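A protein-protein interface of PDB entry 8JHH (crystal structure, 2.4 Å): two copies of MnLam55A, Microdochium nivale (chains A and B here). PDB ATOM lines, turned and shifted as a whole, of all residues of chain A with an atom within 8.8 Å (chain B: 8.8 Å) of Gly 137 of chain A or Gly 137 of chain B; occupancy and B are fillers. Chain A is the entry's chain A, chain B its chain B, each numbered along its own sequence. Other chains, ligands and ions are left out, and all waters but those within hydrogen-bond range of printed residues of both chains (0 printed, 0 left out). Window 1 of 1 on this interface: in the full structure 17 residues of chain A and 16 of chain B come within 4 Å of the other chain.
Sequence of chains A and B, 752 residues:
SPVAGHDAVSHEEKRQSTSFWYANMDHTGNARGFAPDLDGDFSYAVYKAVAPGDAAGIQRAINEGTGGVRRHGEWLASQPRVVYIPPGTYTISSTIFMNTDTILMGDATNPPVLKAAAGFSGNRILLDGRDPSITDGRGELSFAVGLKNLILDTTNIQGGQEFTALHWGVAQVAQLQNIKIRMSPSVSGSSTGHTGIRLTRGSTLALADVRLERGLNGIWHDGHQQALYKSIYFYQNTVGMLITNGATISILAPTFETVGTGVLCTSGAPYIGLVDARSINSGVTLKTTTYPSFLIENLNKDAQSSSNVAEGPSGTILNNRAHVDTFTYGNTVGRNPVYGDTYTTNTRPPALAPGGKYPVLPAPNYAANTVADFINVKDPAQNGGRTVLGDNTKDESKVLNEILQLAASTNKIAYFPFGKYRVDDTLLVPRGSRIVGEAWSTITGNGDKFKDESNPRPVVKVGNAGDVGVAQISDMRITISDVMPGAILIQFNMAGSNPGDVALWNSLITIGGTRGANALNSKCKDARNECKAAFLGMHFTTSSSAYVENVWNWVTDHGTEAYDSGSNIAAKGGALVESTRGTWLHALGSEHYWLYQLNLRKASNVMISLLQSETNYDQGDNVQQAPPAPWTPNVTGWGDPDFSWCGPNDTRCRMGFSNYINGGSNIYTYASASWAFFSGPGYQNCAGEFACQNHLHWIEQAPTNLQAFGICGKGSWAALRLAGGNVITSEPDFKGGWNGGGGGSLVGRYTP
The side-chain carboxylate of Asp 136 of chain A lies within hydrogen-bond range of the backbone NH of Arg 201 of chain B (3.1 Å).
N of Arg 201 of chain A lies within hydrogen-bond range of OD1 of Asp 136 of chain B (3.4 Å).
O of Asp 136 of chain A sits close to O of Asp 136 of chain B (3.4 Å).
The guanidinium group (NH2) of Arg 130 of chain A lies within hydrogen-bond range of the side-chain hydroxyl (OG1) of Thr 200 of chain A.
The guanidinium group (NH2) of Arg 130 of chain A lies within hydrogen-bond range of the backbone carbonyl oxygen (O) of Arg 201 of chain A (2.7 Å).
The backbone carbonyl oxygen (O) of Thr 135 of chain A lies within hydrogen-bond range of the guanidinium group (NE) of Arg 138 of chain A, 2.7 Å away.
OE2 of Glu 140 of chain A is in salt-bridge range of NH2 of Arg 201 of chain A (2.6 Å).
The side-chain hydroxyl of Thr 200 of chain B is in hydrogen-bond range of the guanidinium group of Arg 130 of chain B (3.2 Å).
The guanidinium group (NH1) of Arg 130 of chain B sits at hydrogen-bond distance from the backbone carbonyl oxygen (O) of Arg 201 of chain B, 3.1 Å away.
Thr 135 of chain A touches Thr 200 of chain B.
N of Asp 136 of chain A touches NH2 of Arg 130 of chain B, at 3.8 Å.
O of Gly 137 of chain B touches CA of Asp 136 of chain A, at 3.7 Å.
Asp 136 of chain A touches Thr 200 of chain B (OD1 to CB, 3.3 Å).
Gly 137 of chain A touches Asp 136 of chain B (CA to C, 3.8 Å).
Gly 137 of chain A touches Gly 137 of chain B (N to CA, 3.7 Å).
Asp 136 of chain B touches Thr 200 of chain A.
Arg 201 of chain A touches Arg 201 of chain B (NH1 to NH1, 3.7 Å).
Of chain B, only Asp 136 (3.8 Å) and Gly 137 (3.7 Å) come within 4 Å of Gly 137 of chain A.
Printed residues of chain B within 4 Å of Thr 200 of chain A: Asp 136 (3.2 Å).
Printed residues of chain A within 4 Å of Arg 130 of chain B: Asp 136 (3.8 Å).
Of the printed residues of chain A, Thr 200 of chain B touches Thr 135 and Asp 136.
The nearest residue of chain B that does not touch Gly 137 of chain A is Arg 130 of chain B (4.8 Å).
Along chain B the printed residues that touch a printed residue of chain A span positions 130 to 201.
Printed residues of chain A that touch a printed residue of chain B: Thr 135, Asp 136, Gly 137, Thr 200 and Arg 201.
Along chain A the printed residues that touch a printed residue of chain B span positions 135 to 201.
Among the printed residues, 11 pairs touch across the chains.
Thr 135 of chain A touches Thr 200 of chain B, but with the chains exchanged Thr 200 of chain A does not touch Thr 135 of chain B (4.2 Å).
Asp 136 of chain A touches Arg 130 of chain B, but with the chains exchanged Arg 130 of chain A does not touch Asp 136 of chain B (4.1 Å).
Asp 136 of chain A touches Thr 200 of chain B, and with the chains exchanged Thr 200 of chain A touches Asp 136 of chain B.
Asp 136 of chain A touches Arg 201 of chain B, and with the chains exchanged Arg 201 of chain A touches Asp 136 of chain B.
Positions printed for both chains: 130, 131, 132, 133, 134, 135, 136, 137, 138, 139, 140, 141, 142, 167, 169, 170, 200, 201 and 202.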
ATOM      1  N   GLU A  74       8.923  17.557  23.370  1.00  0.00           N
ATOM      2  CA  GLU A  74       8.290  18.604  22.573  1.00  0.00           C
ATOM      3  C   GLU A  74       9.255  19.320  21.631  1.00  0.00           C
ATOM      4  O   GLU A  74       8.819  20.090  20.770  1.00  0.00           O
ATOM      5  CB  GLU A  74       7.591  19.620  23.487  1.00  0.00           C
ATOM      6  CG  GLU A  74       6.543  19.007  24.409  1.00  0.00           C
ATOM      7  CD  GLU A  74       5.828  20.045  25.259  1.00  0.00           C
ATOM      8  OE1 GLU A  74       6.472  21.029  25.683  1.00  0.00           O
ATOM      9  OE2 GLU A  74       4.612  19.885  25.491  1.00  0.00           O
ATOM     10  N   ARG A 130       2.358   9.762  20.592  1.00  0.00           N
ATOM     11  CA  ARG A 130       2.261  11.085  21.191  1.00  0.00           C
ATOM     12  C   ARG A 130       3.172  11.173  22.412  1.00  0.00           C
ATOM     13  O   ARG A 130       3.124  10.316  23.297  1.00  0.00           O
ATOM     14  CB  ARG A 130       0.809  11.380  21.569  1.00  0.00           C
ATOM     15  CG  ARG A 130       0.546  12.815  22.005  1.00  0.00           C
ATOM     16  CD  ARG A 130      -0.876  12.988  22.524  1.00  0.00           C
ATOM     17  NE  ARG A 130      -1.856  13.129  21.454  1.00  0.00           N
ATOM     18  CZ  ARG A 130      -3.152  12.873  21.585  1.00  0.00           C
ATOM     19  NH1 ARG A 130      -3.659  12.439  22.726  1.00  0.00           N
ATOM     20  NH2 ARG A 130      -3.957  13.048  20.543  1.00  0.00           N
ATOM     21  N   ASP A 131       4.019  12.201  22.443  1.00  0.00           N
ATOM     22  CA  ASP A 131       4.912  12.454  23.570  1.00  0.00           C
ATOM     23  C   ASP A 131       4.101  12.629  24.846  1.00  0.00           C
ATOM     24  O   ASP A 131       3.243  13.511  24.893  1.00  0.00           O
ATOM     25  CB  ASP A 131       5.743  13.708  23.301  1.00  0.00           C
ATOM     26  CG  ASP A 131       6.981  13.800  24.173  1.00  0.00           C
ATOM     27  OD1 ASP A 131       7.016  13.197  25.266  1.00  0.00           O
ATOM     28  OD2 ASP A 131       7.942  14.467  23.741  1.00  0.00           O
ATOM     29  N   PRO A 132       4.318  11.827  25.888  1.00  0.00           N
ATOM     30  CA  PRO A 132       3.538  12.035  27.120  1.00  0.00           C
ATOM     31  C   PRO A 132       3.778  13.395  27.759  1.00  0.00           C
ATOM     32  O   PRO A 132       2.966  13.827  28.585  1.00  0.00           O
ATOM     33  CB  PRO A 132       3.997  10.888  28.036  1.00  0.00           C
ATOM     34  CG  PRO A 132       5.283  10.414  27.466  1.00  0.00           C
ATOM     35  CD  PRO A 132       5.233  10.679  25.994  1.00  0.00           C
ATOM     36  N   SER A 133       4.859  14.087  27.395  1.00  0.00           N
ATOM     37  CA  SER A 133       5.166  15.386  27.979  1.00  0.00           C
ATOM     38  C   SER A 133       4.258  16.507  27.489  1.00  0.00           C
ATOM     39  O   SER A 133       4.259  17.577  28.107  1.00  0.00           O
ATOM     40  CB  SER A 133       6.623  15.757  27.697  1.00  0.00           C
ATOM     41  OG  SER A 133       6.814  16.091  26.335  1.00  0.00           O
ATOM     42  N   ILE A 134       3.495  16.314  26.409  1.00  0.00           N
ATOM     43  CA  ILE A 134       2.552  17.349  26.004  1.00  0.00           C
ATOM     44  C   ILE A 134       1.384  17.377  26.974  1.00  0.00           C
ATOM     45  O   ILE A 134       0.944  16.339  27.486  1.00  0.00           O
ATOM     46  CB  ILE A 134       2.083  17.189  24.540  1.00  0.00           C
ATOM     47  CG1 ILE A 134       1.665  15.768  24.132  1.00  0.00           C
ATOM     48  CG2 ILE A 134       3.175  17.645  23.587  1.00  0.00           C
ATOM     49  CD1 ILE A 134       0.542  15.085  24.900  1.00  0.00           C
ATOM     50  N   THR A 135       0.932  18.574  27.303  1.00  0.00           N
ATOM     51  CA  THR A 135      -0.189  18.704  28.211  1.00  0.00           C
ATOM     52  C   THR A 135      -1.484  18.796  27.416  1.00  0.00           C
ATOM     53  O   THR A 135      -1.515  19.341  26.309  1.00  0.00           O
ATOM     54  CB  THR A 135      -0.018  19.940  29.087  1.00  0.00           C
ATOM     55  OG1 THR A 135       0.388  21.039  28.263  1.00  0.00           O
ATOM     56  CG2 THR A 135       1.047  19.687  30.133  1.00  0.00           C
ATOM     57  N   ASP A 136      -2.552  18.243  27.993  1.00  0.00           N
ATOM     58  CA  ASP A 136      -3.907  18.385  27.460  1.00  0.00           C
ATOM     59  C   ASP A 136      -4.070  17.729  26.091  1.00  0.00           C
ATOM     60  O   ASP A 136      -4.825  18.222  25.248  1.00  0.00           O
ATOM     61  CB  ASP A 136      -4.328  19.856  27.403  1.00  0.00           C
ATOM     62  CG  ASP A 136      -3.888  20.631  28.633  1.00  0.00           C
ATOM     63  OD1 ASP A 136      -3.721  20.005  29.707  1.00  0.00           O
ATOM     64  OD2 ASP A 136      -3.716  21.863  28.528  1.00  0.00           O
ATOM     65  N   GLY A 137      -3.346  16.635  25.865  1.00  0.00           N
ATOM     66  CA  GLY A 137      -3.487  15.811  24.679  1.00  0.00           C
ATOM     67  C   GLY A 137      -3.434  16.550  23.361  1.00  0.00           C
ATOM     68  O   GLY A 137      -4.244  16.290  22.467  1.00  0.00           O
ATOM     69  N   ARG A 138      -2.461  17.444  23.199  1.00  0.00           N
ATOM     70  CA  ARG A 138      -2.370  18.254  21.985  1.00  0.00           C
ATOM     71  C   ARG A 138      -1.478  17.526  20.984  1.00  0.00           C
ATOM     72  O   ARG A 138      -0.282  17.793  20.850  1.00  0.00           O
ATOM     73  CB  ARG A 138      -1.854  19.650  22.312  1.00  0.00           C
ATOM     74  CG  ARG A 138      -2.825  20.479  23.142  1.00  0.00           C
ATOM     75  CD  ARG A 138      -2.139  21.674  23.775  1.00  0.00           C
ATOM     76  NE  ARG A 138      -0.978  21.286  24.565  1.00  0.00           N
ATOM     77  CZ  ARG A 138      -0.085  22.141  25.039  1.00  0.00           C
ATOM     78  NH1 ARG A 138      -0.208  23.443  24.840  1.00  0.00           N
ATOM     79  NH2 ARG A 138       0.969  21.681  25.708  1.00  0.00           N
ATOM     80  N   GLY A 139      -2.099  16.596  20.249  1.00  0.00           N
ATOM     81  CA  GLY A 139      -1.366  15.819  19.263  1.00  0.00           C
ATOM     82  C   GLY A 139      -0.787  16.663  18.148  1.00  0.00           C
ATOM     83  O   GLY A 139       0.229  16.297  17.551  1.00  0.00           O
ATOM     84  N   GLU A 140      -1.396  17.817  17.877  1.00  0.00           N
ATOM     85  CA  GLU A 140      -0.889  18.728  16.860  1.00  0.00           C
ATOM     86  C   GLU A 140       0.475  19.310  17.216  1.00  0.00           C
ATOM     87  O   GLU A 140       1.008  20.102  16.430  1.00  0.00           O
ATOM     88  CB  GLU A 140      -1.890  19.860  16.622  1.00  0.00           C
ATOM     89  CG  GLU A 140      -2.167  20.732  17.835  1.00  0.00           C
ATOM     90  CD  GLU A 140      -3.206  20.137  18.764  1.00  0.00           C
ATOM     91  OE1 GLU A 140      -3.534  18.938  18.611  1.00  0.00           O
ATOM     92  OE2 GLU A 140      -3.691  20.871  19.652  1.00  0.00           O
ATOM     93  N   LEU A 141       1.034  18.964  18.379  1.00  0.00           N
ATOM     94  CA  LEU A 141       2.366  19.400  18.773  1.00  0.00           C
ATOM     95  C   LEU A 141       3.371  18.258  18.829  1.00  0.00           C
ATOM     96  O   LEU A 141       4.561  18.503  19.058  1.00  0.00           O
ATOM     97  CB  LEU A 141       2.304  20.110  20.135  1.00  0.00           C
ATOM     98  CG  LEU A 141       1.549  21.445  20.169  1.00  0.00           C
ATOM     99  CD1 LEU A 141       1.599  22.088  21.542  1.00  0.00           C
ATOM    100  CD2 LEU A 141       2.107  22.391  19.127  1.00  0.00           C
ATOM    101  N   SER A 142       2.930  17.022  18.604  1.00  0.00           N
ATOM    102  CA  SER A 142       3.803  15.850  18.657  1.00  0.00           C
ATOM    103  C   SER A 142       4.464  15.634  17.293  1.00  0.00           C
ATOM    104  O   SER A 142       4.158  14.698  16.550  1.00  0.00           O
ATOM    105  CB  SER A 142       3.007  14.632  19.099  1.00  0.00           C
ATOM    106  OG  SER A 142       3.831  13.489  19.185  1.00  0.00           O
ATOM    107  N   HIS A 167      -1.136   4.100  18.613  1.00  0.00           N
ATOM    108  CA  HIS A 167      -1.871   5.355  18.700  1.00  0.00           C
ATOM    109  C   HIS A 167      -1.075   6.428  17.972  1.00  0.00           C
ATOM    110  O   HIS A 167       0.054   6.743  18.367  1.00  0.00           O
ATOM    111  CB  HIS A 167      -2.125   5.770  20.148  1.00  0.00           C
ATOM    112  CG  HIS A 167      -2.747   7.126  20.272  1.00  0.00           C
ATOM    113  ND1 HIS A 167      -2.040   8.234  20.687  1.00  0.00           N
ATOM    114  CD2 HIS A 167      -4.004   7.557  20.015  1.00  0.00           C
ATOM    115  CE1 HIS A 167      -2.836   9.287  20.688  1.00  0.00           C
ATOM    116  NE2 HIS A 167      -4.034   8.905  20.282  1.00  0.00           N
ATOM    117  N   GLY A 169      -1.966   9.767  17.313  1.00  0.00           N
ATOM    118  CA  GLY A 169      -2.397  11.135  17.514  1.00  0.00           C
ATOM    119  C   GLY A 169      -1.209  12.070  17.537  1.00  0.00           C
ATOM    120  O   GLY A 169      -0.823  12.580  18.593  1.00  0.00           O
ATOM    121  N   VAL A 170      -0.599  12.281  16.372  1.00  0.00           N
ATOM    122  CA  VAL A 170       0.648  13.023  16.276  1.00  0.00           C
ATOM    123  C   VAL A 170       0.479  14.164  15.286  1.00  0.00           C
ATOM    124  O   VAL A 170      -0.633  14.435  14.816  1.00  0.00           O
ATOM    125  CB  VAL A 170       1.804  12.091  15.870  1.00  0.00           C
ATOM    126  CG1 VAL A 170       2.048  11.053  16.957  1.00  0.00           C
ATOM    127  CG2 VAL A 170       1.482  11.409  14.550  1.00  0.00           C
ATOM    128  N   THR A 200      -6.233   9.908  17.062  1.00  0.00           N
ATOM    129  CA  THR A 200      -6.998  10.882  17.818  1.00  0.00           C
ATOM    130  C   THR A 200      -6.476  12.276  17.455  1.00  0.00           C
ATOM    131  O   THR A 200      -5.905  12.466  16.376  1.00  0.00           O
ATOM    132  CB  THR A 200      -6.920  10.552  19.315  1.00  0.00           C
ATOM    133  OG1 THR A 200      -5.565  10.656  19.776  1.00  0.00           O
ATOM    134  CG2 THR A 200      -7.433   9.138  19.572  1.00  0.00           C
ATOM    135  N   ARG A 201      -6.698  13.256  18.333  1.00  0.00           N
ATOM    136  CA  ARG A 201      -6.264  14.633  18.110  1.00  0.00           C
ATOM    137  C   ARG A 201      -4.847  14.686  17.547  1.00  0.00           C
ATOM    138  O   ARG A 201      -3.939  14.016  18.046  1.00  0.00           O
ATOM    139  CB  ARG A 201      -6.347  15.422  19.418  1.00  0.00           C
ATOM    140  CG  ARG A 201      -6.109  16.908  19.257  1.00  0.00           C
ATOM    141  CD  ARG A 201      -6.484  17.686  20.506  1.00  0.00           C
ATOM    142  NE  ARG A 201      -5.961  19.046  20.457  1.00  0.00           N
ATOM    143  CZ  ARG A 201      -6.271  19.998  21.326  1.00  0.00           C
ATOM    144  NH1 ARG A 201      -7.107  19.773  22.325  1.00  0.00           N
ATOM    145  NH2 ARG A 201      -5.728  21.205  21.188  1.00  0.00           N
ATOM    146  N   GLY A 202      -4.677  15.452  16.476  1.00  0.00           N
ATOM    147  CA  GLY A 202      -3.391  15.546  15.815  1.00  0.00           C
ATOM    148  C   GLY A 202      -3.547  16.198  14.464  1.00  0.00           C
ATOM    149  O   GLY A 202      -4.656  16.492  14.011  1.00  0.00           O
ATOM    150  N   ARG B 130      -5.778  11.629  36.105  1.00  0.00           N
ATOM    151  CA  ARG B 130      -6.589  11.642  34.895  1.00  0.00           C
ATOM    152  C   ARG B 130      -6.645  10.253  34.267  1.00  0.00           C
ATOM    153  O   ARG B 130      -5.606   9.635  34.011  1.00  0.00           O
ATOM    154  CB  ARG B 130      -6.036  12.653  33.889  1.00  0.00           C
ATOM    155  CG  ARG B 130      -6.767  12.647  32.547  1.00  0.00           C
ATOM    156  CD  ARG B 130      -6.847  14.039  31.933  1.00  0.00           C
ATOM    157  NE  ARG B 130      -5.632  14.393  31.209  1.00  0.00           N
ATOM    158  CZ  ARG B 130      -5.043  15.581  31.257  1.00  0.00           C
ATOM    159  NH1 ARG B 130      -5.538  16.570  31.978  1.00  0.00           N
ATOM    160  NH2 ARG B 130      -3.931  15.782  30.561  1.00  0.00           N
ATOM    161  N   ASP B 131      -7.859   9.780  34.000  1.00  0.00           N
ATOM    162  CA  ASP B 131      -8.066   8.486  33.361  1.00  0.00           C
ATOM    163  C   ASP B 131      -7.332   8.448  32.025  1.00  0.00           C
ATOM    164  O   ASP B 131      -7.643   9.251  31.133  1.00  0.00           O
ATOM    165  CB  ASP B 131      -9.568   8.258  33.161  1.00  0.00           C
ATOM    166  CG  ASP B 131      -9.920   6.809  32.898  1.00  0.00           C
ATOM    167  OD1 ASP B 131      -9.009   5.993  32.654  1.00  0.00           O
ATOM    168  OD2 ASP B 131     -11.122   6.482  32.950  1.00  0.00           O
ATOM    169  N   PRO B 132      -6.356   7.553  31.841  1.00  0.00           N
ATOM    170  CA  PRO B 132      -5.656   7.493  30.550  1.00  0.00           C
ATOM    171  C   PRO B 132      -6.546   7.070  29.397  1.00  0.00           C
ATOM    172  O   PRO B 132      -6.202   7.345  28.241  1.00  0.00           O
ATOM    173  CB  PRO B 132      -4.544   6.466  30.800  1.00  0.00           C
ATOM    174  CG  PRO B 132      -5.073   5.612  31.897  1.00  0.00           C
ATOM    175  CD  PRO B 132      -5.854   6.541  32.784  1.00  0.00           C
ATOM    176  N   SER B 133      -7.680   6.423  29.670  1.00  0.00           N
ATOM    177  CA  SER B 133      -8.571   6.003  28.599  1.00  0.00           C
ATOM    178  C   SER B 133      -9.325   7.168  27.985  1.00  0.00           C
ATOM    179  O   SER B 133      -9.903   7.009  26.906  1.00  0.00           O
ATOM    180  CB  SER B 133      -9.564   4.965  29.113  1.00  0.00           C
ATOM    181  OG  SER B 133     -10.562   5.586  29.898  1.00  0.00           O
ATOM    182  N   ILE B 134      -9.336   8.328  28.640  1.00  0.00           N
ATOM    183  CA  ILE B 134      -9.926   9.511  28.033  1.00  0.00           C
ATOM    184  C   ILE B 134      -9.002   9.997  26.927  1.00  0.00           C
ATOM    185  O   ILE B 134      -7.780  10.086  27.107  1.00  0.00           O
ATOM    186  CB  ILE B 134     -10.161  10.597  29.093  1.00  0.00           C
ATOM    187  CG1 ILE B 134     -11.083  10.065  30.193  1.00  0.00           C
ATOM    188  CG2 ILE B 134     -10.732  11.858  28.452  1.00  0.00           C
ATOM    189  CD1 ILE B 134     -11.873  11.125  30.907  1.00  0.00           C
ATOM    190  N   THR B 135      -9.582  10.338  25.786  1.00  0.00           N
ATOM    191  CA  THR B 135      -8.817  10.756  24.624  1.00  0.00           C
ATOM    192  C   THR B 135      -8.655  12.270  24.582  1.00  0.00           C
ATOM    193  O   THR B 135      -9.493  13.022  25.090  1.00  0.00           O
ATOM    194  CB  THR B 135      -9.487  10.270  23.338  1.00  0.00           C
ATOM    195  OG1 THR B 135     -10.844  10.729  23.304  1.00  0.00           O
ATOM    196  CG2 THR B 135      -9.469   8.755  23.275  1.00  0.00           C
ATOM    197  N   ASP B 136      -7.539  12.703  23.992  1.00  0.00           N
ATOM    198  CA  ASP B 136      -7.271  14.109  23.701  1.00  0.00           C
ATOM    199  C   ASP B 136      -7.132  14.948  24.967  1.00  0.00           C
ATOM    200  O   ASP B 136      -7.450  16.139  24.960  1.00  0.00           O
ATOM    201  CB  ASP B 136      -8.349  14.708  22.786  1.00  0.00           C
ATOM    202  CG  ASP B 136      -8.696  13.799  21.620  1.00  0.00           C
ATOM    203  OD1 ASP B 136      -7.974  12.805  21.406  1.00  0.00           O
ATOM    204  OD2 ASP B 136      -9.684  14.078  20.910  1.00  0.00           O
ATOM    205  N   GLY B 137      -6.633  14.335  26.043  1.00  0.00           N
ATOM    206  CA  GLY B 137      -6.334  15.030  27.281  1.00  0.00           C
ATOM    207  C   GLY B 137      -7.479  15.857  27.825  1.00  0.00           C
ATOM    208  O   GLY B 137      -7.301  17.034  28.150  1.00  0.00           O
ATOM    209  N   ARG B 138      -8.673  15.268  27.893  1.00  0.00           N
ATOM    210  CA  ARG B 138      -9.865  15.987  28.342  1.00  0.00           C
ATOM    211  C   ARG B 138     -10.074  15.740  29.835  1.00  0.00           C
ATOM    212  O   ARG B 138     -10.836  14.869  30.262  1.00  0.00           O
ATOM    213  CB  ARG B 138     -11.071  15.571  27.507  1.00  0.00           C
ATOM    214  CG  ARG B 138     -10.891  15.828  26.013  1.00  0.00           C
ATOM    215  CD  ARG B 138     -12.104  15.379  25.215  1.00  0.00           C
ATOM    216  NE  ARG B 138     -12.179  13.926  25.107  1.00  0.00           N
ATOM    217  CZ  ARG B 138     -13.263  13.258  24.732  1.00  0.00           C
ATOM    218  NH1 ARG B 138     -14.382  13.882  24.405  1.00  0.00           N
ATOM    219  NH2 ARG B 138     -13.226  11.928  24.695  1.00  0.00           N
ATOM    220  N   GLY B 139      -9.373  16.540  30.645  1.00  0.00           N
ATOM    221  CA  GLY B 139      -9.497  16.420  32.086  1.00  0.00           C
ATOM    222  C   GLY B 139     -10.883  16.748  32.601  1.00  0.00           C
ATOM    223  O   GLY B 139     -11.297  16.242  33.645  1.00  0.00           O
ATOM    224  N   GLU B 140     -11.629  17.578  31.868  1.00  0.00           N
ATOM    225  CA  GLU B 140     -12.985  17.938  32.262  1.00  0.00           C
ATOM    226  C   GLU B 140     -13.955  16.764  32.225  1.00  0.00           C
ATOM    227  O   GLU B 140     -15.126  16.940  32.583  1.00  0.00           O
ATOM    228  CB  GLU B 140     -13.499  19.060  31.367  1.00  0.00           C
ATOM    229  CG  GLU B 140     -13.776  18.641  29.938  1.00  0.00           C
ATOM    230  CD  GLU B 140     -12.595  18.872  29.020  1.00  0.00           C
ATOM    231  OE1 GLU B 140     -11.450  18.937  29.520  1.00  0.00           O
ATOM    232  OE2 GLU B 140     -12.813  18.990  27.794  1.00  0.00           O
ATOM    233  N   LEU B 141     -13.509  15.583  31.800  1.00  0.00           N
ATOM    234  CA  LEU B 141     -14.333  14.385  31.812  1.00  0.00           C
ATOM    235  C   LEU B 141     -13.845  13.362  32.824  1.00  0.00           C
ATOM    236  O   LEU B 141     -14.490  12.320  32.994  1.00  0.00           O
ATOM    237  CB  LEU B 141     -14.380  13.761  30.411  1.00  0.00           C
ATOM    238  CG  LEU B 141     -14.980  14.615  29.291  1.00  0.00           C
ATOM    239  CD1 LEU B 141     -14.847  13.920  27.940  1.00  0.00           C
ATOM    240  CD2 LEU B 141     -16.440  14.937  29.588  1.00  0.00           C
ATOM    241  N   SER B 142     -12.737  13.635  33.513  1.00  0.00           N
ATOM    242  CA  SER B 142     -12.167  12.695  34.475  1.00  0.00           C
ATOM    243  C   SER B 142     -12.849  12.883  35.830  1.00  0.00           C
ATOM    244  O   SER B 142     -12.280  13.398  36.793  1.00  0.00           O
ATOM    245  CB  SER B 142     -10.658  12.882  34.567  1.00  0.00           C
ATOM    246  OG  SER B 142     -10.048  11.877  35.365  1.00  0.00           O
ATOM    247  N   HIS B 167      -0.540  14.524  39.296  1.00  0.00           N
ATOM    248  CA  HIS B 167      -1.156  15.274  38.212  1.00  0.00           C
ATOM    249  C   HIS B 167      -2.662  15.254  38.422  1.00  0.00           C
ATOM    250  O   HIS B 167      -3.280  14.187  38.393  1.00  0.00           O
ATOM    251  CB  HIS B 167      -0.788  14.681  36.853  1.00  0.00           C
ATOM    252  CG  HIS B 167      -1.414  15.398  35.702  1.00  0.00           C
ATOM    253  ND1 HIS B 167      -2.448  14.862  34.965  1.00  0.00           N
ATOM    254  CD2 HIS B 167      -1.165  16.617  35.170  1.00  0.00           C
ATOM    255  CE1 HIS B 167      -2.805  15.718  34.026  1.00  0.00           C
ATOM    256  NE2 HIS B 167      -2.042  16.791  34.128  1.00  0.00           N
ATOM    257  N   GLY B 169      -5.160  16.980  36.655  1.00  0.00           N
ATOM    258  CA  GLY B 169      -5.982  17.472  35.569  1.00  0.00           C
ATOM    259  C   GLY B 169      -7.260  16.668  35.486  1.00  0.00           C
ATOM    260  O   GLY B 169      -7.431  15.859  34.569  1.00  0.00           O
ATOM    261  N   VAL B 170      -8.156  16.865  36.455  1.00  0.00           N
ATOM    262  CA  VAL B 170      -9.343  16.028  36.599  1.00  0.00           C
ATOM    263  C   VAL B 170     -10.595  16.893  36.589  1.00  0.00           C
ATOM    264  O   VAL B 170     -10.528  18.104  36.351  1.00  0.00           O
ATOM    265  CB  VAL B 170      -9.273  15.182  37.885  1.00  0.00           C
ATOM    266  CG1 VAL B 170      -8.144  14.165  37.794  1.00  0.00           C
ATOM    267  CG2 VAL B 170      -9.100  16.078  39.104  1.00  0.00           C
ATOM    268  N   THR B 200      -3.540  20.563  35.161  1.00  0.00           N
ATOM    269  CA  THR B 200      -3.664  20.920  33.758  1.00  0.00           C
ATOM    270  C   THR B 200      -5.148  20.977  33.404  1.00  0.00           C
ATOM    271  O   THR B 200      -5.996  21.154  34.286  1.00  0.00           O
ATOM    272  CB  THR B 200      -2.867  19.934  32.900  1.00  0.00           C
ATOM    273  OG1 THR B 200      -3.325  18.597  33.142  1.00  0.00           O
ATOM    274  CG2 THR B 200      -1.388  20.029  33.229  1.00  0.00           C
ATOM    275  N   ARG B 201      -5.470  20.852  32.116  1.00  0.00           N
ATOM    276  CA  ARG B 201      -6.848  20.874  31.637  1.00  0.00           C
ATOM    277  C   ARG B 201      -7.748  20.024  32.525  1.00  0.00           C
ATOM    278  O   ARG B 201      -7.420  18.880  32.847  1.00  0.00           O
ATOM    279  CB  ARG B 201      -6.903  20.373  30.193  1.00  0.00           C
ATOM    280  CG  ARG B 201      -8.297  20.216  29.632  1.00  0.00           C
ATOM    281  CD  ARG B 201      -8.277  20.190  28.117  1.00  0.00           C
ATOM    282  NE  ARG B 201      -9.618  20.087  27.555  1.00  0.00           N
ATOM    283  CZ  ARG B 201      -9.907  20.266  26.274  1.00  0.00           C
ATOM    284  NH1 ARG B 201      -8.967  20.564  25.390  1.00  0.00           N
ATOM    285  NH2 ARG B 201     -11.168  20.142  25.868  1.00  0.00           N
ATOM    286  N   GLY B 202      -8.864  20.609  32.949  1.00  0.00           N
ATOM    287  CA  GLY B 202      -9.790  19.929  33.835  1.00  0.00           C
ATOM    288  C   GLY B 202     -10.769  20.917  34.426  1.00  0.00           C
ATOM    289  O   GLY B 202     -10.665  22.127  34.233  1.00  0.00           O
